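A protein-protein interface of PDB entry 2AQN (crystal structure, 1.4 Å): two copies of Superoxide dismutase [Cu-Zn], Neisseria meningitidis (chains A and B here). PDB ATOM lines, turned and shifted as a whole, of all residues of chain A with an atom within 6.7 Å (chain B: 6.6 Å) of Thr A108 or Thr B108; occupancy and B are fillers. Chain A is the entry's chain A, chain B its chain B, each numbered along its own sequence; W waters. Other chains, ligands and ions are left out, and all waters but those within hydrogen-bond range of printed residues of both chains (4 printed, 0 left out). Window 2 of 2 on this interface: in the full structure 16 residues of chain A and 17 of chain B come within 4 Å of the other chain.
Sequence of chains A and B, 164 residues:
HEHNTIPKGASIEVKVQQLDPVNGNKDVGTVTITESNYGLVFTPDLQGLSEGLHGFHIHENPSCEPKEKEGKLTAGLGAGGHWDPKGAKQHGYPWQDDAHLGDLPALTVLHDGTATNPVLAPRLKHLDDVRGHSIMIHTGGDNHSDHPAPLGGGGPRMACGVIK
Among the printed residues, pairs that only touch across the chains: Leu A53 with Asn B117, Asn A117 with Leu B53, Leu A110 with Leu B53, Asn A117 with Ala B106 and Leu A110 with Gly B52.
Water W1 lies within hydrogen-bond range of O of Ala A106 (2.8 Å) and OD1 of Asn B117 (2.9 Å).
Water W3 bridges O of Ala B106 (2.8 Å) and OD1 of Asn A117 (2.9 Å).
Water W2 bridges ND2 of Asn A117 (2.8 Å) and N of Ala B106 (3.0 Å).
Water W4 lies within hydrogen-bond range of ND2 of Asn B117 and N of Ala A106.
OG1 of Thr A108 sits at hydrogen-bond distance from OG1 of Thr B108 (2.7 Å).
Thr A108 touches just one residue of chain B: Thr B108.
Printed residues of chain B within 4 Å of Leu A110: Gly B52 (3.97 Å) and Leu B53 (3.9 Å).
Of chain A, only Thr A108 (2.7 Å) comes within 4 Å of Thr B108.
Of the printed residues of chain A, Asn B117 touches Leu A53.
The nearest residue of chain A that does not touch Thr B108 is Leu A53 (4.2 Å).
Leu A53 touches Asn B117, and with the chains exchanged Asn A117 touches Leu B53.
Thr B108 touches its own counterpart, Thr A108.
Leu A110 touches Gly B52, but with the chains exchanged Gly A52 does not touch Leu B110 (4.4 Å).
Leu A110 touches Leu B53, but with the chains exchanged Leu A53 does not touch Leu B110 (4.003 Å).
Positions printed for both chains: 44, 52, 53, 54, 106, 107, 108, 109, 110, 114, 115, 116, 117 and 119.
Hydrophobic or aromatic side chains of chain B within 4 Å of the printed part of chain A: Leu B53 and Ala B106.
Printed residues of chain A that touch a printed residue of chain B: Leu A53, Thr A108, Leu A110 and Asn A117.
Hydrophobic or aromatic side chains of chain A that line the printed part of chain B: Leu A53 and Leu A110.
Among the printed residues, 6 pairs touch across the chains.
The backbone carbonyl oxygen (O) of Gly B52 lies within hydrogen-bond range of the backbone NH (N) of Val B109, 2.9 Å away.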
ATOM      1  N   PRO A  44      10.862  -0.895   1.847  1.00  0.00           N
ATOM      2  CA  PRO A  44      11.086  -0.718   3.278  1.00  0.00           C
ATOM      3  C   PRO A  44      11.673  -1.978   3.884  1.00  0.00           C
ATOM      4  O   PRO A  44      11.475  -3.091   3.368  1.00  0.00           O
ATOM      5  CB  PRO A  44       9.668  -0.487   3.774  1.00  0.00           C
ATOM      6  CG  PRO A  44       8.806  -1.289   2.874  1.00  0.00           C
ATOM      7  CD  PRO A  44       9.473  -1.251   1.521  1.00  0.00           C
ATOM      8  N   SER A  50       3.221   0.635  14.142  1.00  0.00           N
ATOM      9  CA  SER A  50       1.864   0.244  14.422  1.00  0.00           C
ATOM     10  C   SER A  50       1.181  -0.380  13.196  1.00  0.00           C
ATOM     11  O   SER A  50       1.377   0.055  12.064  1.00  0.00           O
ATOM     12  CB  SER A  50       1.031   1.422  14.942  1.00  0.00           C
ATOM     13  OG  SER A  50       0.974   2.413  13.953  1.00  0.00           O
ATOM     14  N   GLY A  52      -1.114  -1.288  10.259  1.00  0.00           N
ATOM     15  CA  GLY A  52      -2.028  -0.529   9.434  1.00  0.00           C
ATOM     16  C   GLY A  52      -1.349   0.024   8.201  1.00  0.00           C
ATOM     17  O   GLY A  52      -0.174  -0.184   7.969  1.00  0.00           O
ATOM     18  N   LEU A  53      -2.141   0.746   7.427  1.00  0.00           N
ATOM     19  CA  LEU A  53      -1.632   1.540   6.337  1.00  0.00           C
ATOM     20  C   LEU A  53      -1.238   2.911   6.855  1.00  0.00           C
ATOM     21  O   LEU A  53      -1.931   3.530   7.650  1.00  0.00           O
ATOM     22  CB  LEU A  53      -2.726   1.678   5.292  1.00  0.00           C
ATOM     23  CG  LEU A  53      -2.963   0.444   4.428  1.00  0.00           C
ATOM     24  CD1 LEU A  53      -4.321   0.439   3.783  1.00  0.00           C
ATOM     25  CD2 LEU A  53      -1.846   0.370   3.358  1.00  0.00           C
ATOM     26  N   HIS A  54      -0.061   3.389   6.465  1.00  0.00           N
ATOM     27  CA  HIS A  54       0.433   4.674   6.900  1.00  0.00           C
ATOM     28  C   HIS A  54       0.772   5.602   5.730  1.00  0.00           C
ATOM     29  O   HIS A  54       1.393   5.162   4.725  1.00  0.00           O
ATOM     30  CB  HIS A  54       1.710   4.488   7.717  1.00  0.00           C
ATOM     31  CG  HIS A  54       1.479   3.797   8.996  1.00  0.00           C
ATOM     32  ND1 HIS A  54       1.212   4.486  10.153  1.00  0.00           N
ATOM     33  CD2 HIS A  54       1.477   2.469   9.283  1.00  0.00           C
ATOM     34  CE1 HIS A  54       1.045   3.572  11.102  1.00  0.00           C
ATOM     35  NE2 HIS A  54       1.199   2.347  10.615  1.00  0.00           N
ATOM     36  N   PRO A 105       2.690   5.813  -2.621  1.00  0.00           N
ATOM     37  CA  PRO A 105       1.681   4.854  -2.169  1.00  0.00           C
ATOM     38  C   PRO A 105       1.801   4.681  -0.665  1.00  0.00           C
ATOM     39  O   PRO A 105       2.893   4.800  -0.102  1.00  0.00           O
ATOM     40  CB  PRO A 105       2.104   3.552  -2.848  1.00  0.00           C
ATOM     41  CG  PRO A 105       2.894   4.012  -4.061  1.00  0.00           C
ATOM     42  CD  PRO A 105       3.666   5.185  -3.542  1.00  0.00           C
ATOM     43  N   ALA A 106       0.708   4.349   0.016  1.00  0.00           N
ATOM     44  CA  ALA A 106       0.750   4.093   1.436  1.00  0.00           C
ATOM     45  C   ALA A 106       1.617   2.877   1.744  1.00  0.00           C
ATOM     46  O   ALA A 106       1.727   1.922   0.972  1.00  0.00           O
ATOM     47  CB  ALA A 106      -0.641   3.927   2.025  1.00  0.00           C
ATOM     48  N   LEU A 107       2.259   2.968   2.900  1.00  0.00           N
ATOM     49  CA  LEU A 107       3.115   1.928   3.464  1.00  0.00           C
ATOM     50  C   LEU A 107       2.293   0.936   4.270  1.00  0.00           C
ATOM     51  O   LEU A 107       1.481   1.319   5.123  1.00  0.00           O
ATOM     52  CB  LEU A 107       4.132   2.613   4.397  1.00  0.00           C
ATOM     53  CG  LEU A 107       5.123   1.652   5.054  1.00  0.00           C
ATOM     54  CD1 LEU A 107       6.138   1.195   4.035  1.00  0.00           C
ATOM     55  CD2 LEU A 107       5.802   2.344   6.220  1.00  0.00           C
ATOM     56  N   THR A 108       2.496  -0.345   4.048  1.00  0.00           N
ATOM     57  CA  THR A 108       1.818  -1.388   4.810  1.00  0.00           C
ATOM     58  C   THR A 108       2.658  -1.908   5.961  1.00  0.00           C
ATOM     59  O   THR A 108       3.762  -2.387   5.754  1.00  0.00           O
ATOM     60  CB  THR A 108       1.490  -2.587   3.905  1.00  0.00           C
ATOM     61  OG1 THR A 108       0.556  -2.181   2.919  1.00  0.00           O
ATOM     62  CG2 THR A 108       0.837  -3.709   4.694  1.00  0.00           C
ATOM     63  N   VAL A 109       2.121  -1.801   7.169  1.00  0.00           N
ATOM     64  CA  VAL A 109       2.746  -2.347   8.360  1.00  0.00           C
ATOM     65  C   VAL A 109       1.876  -3.514   8.842  1.00  0.00           C
ATOM     66  O   VAL A 109       0.674  -3.327   9.079  1.00  0.00           O
ATOM     67  CB  VAL A 109       2.904  -1.314   9.485  1.00  0.00           C
ATOM     68  CG1 VAL A 109       3.522  -1.997  10.672  1.00  0.00           C
ATOM     69  CG2 VAL A 109       3.756  -0.152   8.986  1.00  0.00           C
ATOM     70  N   LEU A 110       2.431  -4.698   8.953  1.00  0.00           N
ATOM     71  CA  LEU A 110       1.680  -5.888   9.351  1.00  0.00           C
ATOM     72  C   LEU A 110       1.420  -5.909  10.854  1.00  0.00           C
ATOM     73  O   LEU A 110       1.913  -5.094  11.621  1.00  0.00           O
ATOM     74  CB  LEU A 110       2.465  -7.137   8.920  1.00  0.00           C
ATOM     75  CG  LEU A 110       2.679  -7.286   7.411  1.00  0.00           C
ATOM     76  CD1 LEU A 110       3.474  -8.533   7.056  1.00  0.00           C
ATOM     77  CD2 LEU A 110       1.341  -7.347   6.659  1.00  0.00           C
ATOM     78  N   THR A 114       6.124  -4.954  11.228  1.00  0.00           N
ATOM     79  CA  THR A 114       7.092  -4.846  10.164  1.00  0.00           C
ATOM     80  C   THR A 114       6.467  -4.374   8.846  1.00  0.00           C
ATOM     81  O   THR A 114       5.301  -4.547   8.495  1.00  0.00           O
ATOM     82  CB  THR A 114       7.794  -6.190   9.906  1.00  0.00           C
ATOM     83  OG1 THR A 114       6.809  -7.105   9.377  1.00  0.00           O
ATOM     84  CG2 THR A 114       8.365  -6.804  11.166  1.00  0.00           C
ATOM     85  N   ALA A 115       7.337  -3.749   8.048  1.00  0.00           N
ATOM     86  CA  ALA A 115       7.088  -3.322   6.700  1.00  0.00           C
ATOM     87  C   ALA A 115       8.222  -3.713   5.754  1.00  0.00           C
ATOM     88  O   ALA A 115       9.325  -3.207   5.949  1.00  0.00           O
ATOM     89  CB  ALA A 115       6.837  -1.823   6.663  1.00  0.00           C
ATOM     90  N   THR A 116       7.914  -4.563   4.782  1.00  0.00           N
ATOM     91  CA  THR A 116       8.834  -4.997   3.740  1.00  0.00           C
ATOM     92  C   THR A 116       8.254  -4.873   2.331  1.00  0.00           C
ATOM     93  O   THR A 116       8.968  -5.186   1.370  1.00  0.00           O
ATOM     94  CB  THR A 116       9.238  -6.477   3.935  1.00  0.00           C
ATOM     95  OG1 THR A 116       8.047  -7.288   3.889  1.00  0.00           O
ATOM     96  CG2 THR A 116       9.875  -6.731   5.285  1.00  0.00           C
ATOM     97  N   ASN A 117       7.001  -4.450   2.180  1.00  0.00           N
ATOM     98  CA  ASN A 117       6.403  -4.433   0.852  1.00  0.00           C
ATOM     99  C   ASN A 117       6.861  -3.229   0.046  1.00  0.00           C
ATOM    100  O   ASN A 117       6.592  -2.107   0.456  1.00  0.00           O
ATOM    101  CB  ASN A 117       4.860  -4.471   0.989  1.00  0.00           C
ATOM    102  CG  ASN A 117       4.124  -4.486  -0.313  1.00  0.00           C
ATOM    103  OD1 ASN A 117       3.252  -3.625  -0.580  1.00  0.00           O
ATOM    104  ND2 ASN A 117       4.478  -5.401  -1.171  1.00  0.00           N
ATOM    105  N   VAL A 119       6.956  -0.269  -2.872  1.00  0.00           N
ATOM    106  CA  VAL A 119       5.932   0.471  -3.579  1.00  0.00           C
ATOM    107  C   VAL A 119       6.595   1.363  -4.625  1.00  0.00           C
ATOM    108  O   VAL A 119       7.743   1.812  -4.430  1.00  0.00           O
ATOM    109  CB  VAL A 119       5.060   1.320  -2.632  1.00  0.00           C
ATOM    110  CG1 VAL A 119       4.248   0.493  -1.614  1.00  0.00           C
ATOM    111  CG2 VAL A 119       5.876   2.372  -1.855  1.00  0.00           C
ATOM    112  N   PRO B  44      -9.556  -2.088  -4.583  1.00  0.00           N
ATOM    113  CA  PRO B  44     -10.344  -3.124  -3.944  1.00  0.00           C
ATOM    114  C   PRO B  44     -11.406  -2.490  -3.037  1.00  0.00           C
ATOM    115  O   PRO B  44     -11.251  -1.385  -2.535  1.00  0.00           O
ATOM    116  CB  PRO B  44      -9.353  -3.896  -3.075  1.00  0.00           C
ATOM    117  CG  PRO B  44      -8.323  -2.855  -2.731  1.00  0.00           C
ATOM    118  CD  PRO B  44      -8.288  -1.879  -3.872  1.00  0.00           C
ATOM    119  N   GLY B  52      -3.263  -9.366   6.236  1.00  0.00           N
ATOM    120  CA  GLY B  52      -1.899  -9.443   5.735  1.00  0.00           C
ATOM    121  C   GLY B  52      -1.764  -9.009   4.303  1.00  0.00           C
ATOM    122  O   GLY B  52      -2.705  -8.545   3.677  1.00  0.00           O
ATOM    123  N   LEU B  53      -0.560  -9.193   3.788  1.00  0.00           N
ATOM    124  CA  LEU B  53      -0.261  -8.998   2.386  1.00  0.00           C
ATOM    125  C   LEU B  53      -0.598 -10.276   1.612  1.00  0.00           C
ATOM    126  O   LEU B  53      -0.259 -11.384   2.063  1.00  0.00           O
ATOM    127  CB  LEU B  53       1.191  -8.666   2.182  1.00  0.00           C
ATOM    128  CG  LEU B  53       1.600  -7.277   2.633  1.00  0.00           C
ATOM    129  CD1 LEU B  53       3.090  -7.244   2.942  1.00  0.00           C
ATOM    130  CD2 LEU B  53       1.230  -6.272   1.534  1.00  0.00           C
ATOM    131  N   HIS B  54      -1.264 -10.107   0.482  1.00  0.00           N
ATOM    132  CA  HIS B  54      -1.695 -11.250  -0.323  1.00  0.00           C
ATOM    133  C   HIS B  54      -1.230 -11.067  -1.738  1.00  0.00           C
ATOM    134  O   HIS B  54      -1.450 -10.024  -2.338  1.00  0.00           O
ATOM    135  CB  HIS B  54      -3.217 -11.378  -0.284  1.00  0.00           C
ATOM    136  CG  HIS B  54      -3.713 -11.814   1.078  1.00  0.00           C
ATOM    137  ND1 HIS B  54      -3.678 -13.130   1.488  1.00  0.00           N
ATOM    138  CD2 HIS B  54      -4.192 -11.106   2.128  1.00  0.00           C
ATOM    139  CE1 HIS B  54      -4.154 -13.214   2.729  1.00  0.00           C
ATOM    140  NE2 HIS B  54      -4.476 -11.996   3.144  1.00  0.00           N
ATOM    141  N   ALA B 106       1.094  -6.436  -4.462  1.00  0.00           N
ATOM    142  CA  ALA B 106       0.415  -7.183  -3.416  1.00  0.00           C
ATOM    143  C   ALA B 106      -0.741  -6.358  -2.821  1.00  0.00           C
ATOM    144  O   ALA B 106      -0.703  -5.126  -2.686  1.00  0.00           O
ATOM    145  CB  ALA B 106       1.416  -7.603  -2.351  1.00  0.00           C
ATOM    146  N   LEU B 107      -1.808  -7.075  -2.440  1.00  0.00           N
ATOM    147  CA  LEU B 107      -2.977  -6.464  -1.806  1.00  0.00           C
ATOM    148  C   LEU B 107      -2.810  -6.478  -0.292  1.00  0.00           C
ATOM    149  O   LEU B 107      -2.309  -7.463   0.254  1.00  0.00           O
ATOM    150  CB  LEU B 107      -4.220  -7.262  -2.159  1.00  0.00           C
ATOM    151  CG  LEU B 107      -5.073  -6.914  -3.344  1.00  0.00           C
ATOM    152  CD1 LEU B 107      -6.381  -7.716  -3.231  1.00  0.00           C
ATOM    153  CD2 LEU B 107      -5.367  -5.429  -3.489  1.00  0.00           C
ATOM    154  N   THR B 108      -3.237  -5.407   0.370  1.00  0.00           N
ATOM    155  CA  THR B 108      -3.189  -5.278   1.803  1.00  0.00           C
ATOM    156  C   THR B 108      -4.587  -5.501   2.374  1.00  0.00           C
ATOM    157  O   THR B 108      -5.508  -4.784   2.009  1.00  0.00           O
ATOM    158  CB  THR B 108      -2.672  -3.887   2.226  1.00  0.00           C
ATOM    159  OG1 THR B 108      -1.331  -3.768   1.791  1.00  0.00           O
ATOM    160  CG2 THR B 108      -2.757  -3.721   3.737  1.00  0.00           C
ATOM    161  N   VAL B 109      -4.700  -6.519   3.234  1.00  0.00           N
ATOM    162  CA  VAL B 109      -5.916  -6.730   3.999  1.00  0.00           C
ATOM    163  C   VAL B 109      -5.612  -6.322   5.432  1.00  0.00           C
ATOM    164  O   VAL B 109      -4.693  -6.839   6.061  1.00  0.00           O
ATOM    165  CB  VAL B 109      -6.405  -8.192   3.931  1.00  0.00           C
ATOM    166  CG1 VAL B 109      -7.631  -8.369   4.825  1.00  0.00           C
ATOM    167  CG2 VAL B 109      -6.650  -8.579   2.489  1.00  0.00           C
ATOM    168  N   LEU B 110      -6.408  -5.404   5.972  1.00  0.00           N
ATOM    169  CA  LEU B 110      -6.245  -4.934   7.328  1.00  0.00           C
ATOM    170  C   LEU B 110      -6.722  -5.925   8.379  1.00  0.00           C
ATOM    171  O   LEU B 110      -7.318  -6.945   8.032  1.00  0.00           O
ATOM    172  CB  LEU B 110      -7.007  -3.604   7.484  1.00  0.00           C
ATOM    173  CG  LEU B 110      -6.537  -2.489   6.559  1.00  0.00           C
ATOM    174  CD1 LEU B 110      -7.388  -1.259   6.846  1.00  0.00           C
ATOM    175  CD2 LEU B 110      -5.048  -2.196   6.707  1.00  0.00           C
ATOM    176  N   THR B 114     -10.647  -6.195   5.817  1.00  0.00           N
ATOM    177  CA  THR B 114     -11.004  -5.429   4.647  1.00  0.00           C
ATOM    178  C   THR B 114      -9.802  -5.001   3.825  1.00  0.00           C
ATOM    179  O   THR B 114      -8.697  -4.883   4.330  1.00  0.00           O
ATOM    180  CB  THR B 114     -11.803  -4.162   5.015  1.00  0.00           C
ATOM    181  OG1 THR B 114     -11.014  -3.251   5.803  1.00  0.00           O
ATOM    182  CG2 THR B 114     -13.017  -4.589   5.849  1.00  0.00           C
ATOM    183  N   ALA B 115     -10.059  -4.746   2.556  1.00  0.00           N
ATOM    184  CA  ALA B 115      -9.043  -4.176   1.678  1.00  0.00           C
ATOM    185  C   ALA B 115      -9.680  -3.081   0.843  1.00  0.00           C
ATOM    186  O   ALA B 115     -10.625  -3.362   0.088  1.00  0.00           O
ATOM    187  CB  ALA B 115      -8.453  -5.300   0.875  1.00  0.00           C
ATOM    188  N   THR B 116      -9.148  -1.872   0.967  1.00  0.00           N
ATOM    189  CA  THR B 116      -9.570  -0.739   0.144  1.00  0.00           C
ATOM    190  C   THR B 116      -8.432   0.078  -0.455  1.00  0.00           C
ATOM    191  O   THR B 116      -8.694   1.097  -1.107  1.00  0.00           O
ATOM    192  CB  THR B 116     -10.469   0.227   0.943  1.00  0.00           C
ATOM    193  OG1 THR B 116      -9.791   0.679   2.122  1.00  0.00           O
ATOM    194  CG2 THR B 116     -11.730  -0.454   1.441  1.00  0.00           C
ATOM    195  N   ASN B 117      -7.186  -0.298  -0.245  1.00  0.00           N
ATOM    196  CA  ASN B 117      -6.033   0.473  -0.735  1.00  0.00           C
ATOM    197  C   ASN B 117      -5.780   0.164  -2.204  1.00  0.00           C
ATOM    198  O   ASN B 117      -5.501  -0.981  -2.569  1.00  0.00           O
ATOM    199  CB  ASN B 117      -4.827   0.149   0.117  1.00  0.00           C
ATOM    200  CG  ASN B 117      -3.548   0.873  -0.264  1.00  0.00           C
ATOM    201  OD1 ASN B 117      -2.492   0.243  -0.503  1.00  0.00           O
ATOM    202  ND2 ASN B 117      -3.648   2.179  -0.332  1.00  0.00           N
ATOM    203  N   VAL B 119      -3.884  -0.096  -5.906  1.00  0.00           N
ATOM    204  CA  VAL B 119      -2.546  -0.370  -6.381  1.00  0.00           C
ATOM    205  C   VAL B 119      -2.481  -0.158  -7.903  1.00  0.00           C
ATOM    206  O   VAL B 119      -3.451  -0.394  -8.639  1.00  0.00           O
ATOM    207  CB  VAL B 119      -2.065  -1.785  -5.987  1.00  0.00           C
ATOM    208  CG1 VAL B 119      -2.043  -1.965  -4.471  1.00  0.00           C
ATOM    209  CG2 VAL B 119      -2.907  -2.882  -6.628  1.00  0.00           C
HETATM  210  O   HOH W   1       0.197   1.158  -1.205  1.00  0.00           O
HETATM  211  O   HOH W   2       3.852  -5.514  -3.913  1.00  0.00           O
HETATM  212  O   HOH W   3       1.438  -3.355  -2.815  1.00  0.00           O
HETATM  213  O   HOH W   4      -1.743   3.909  -1.482  1.00  0.00           O
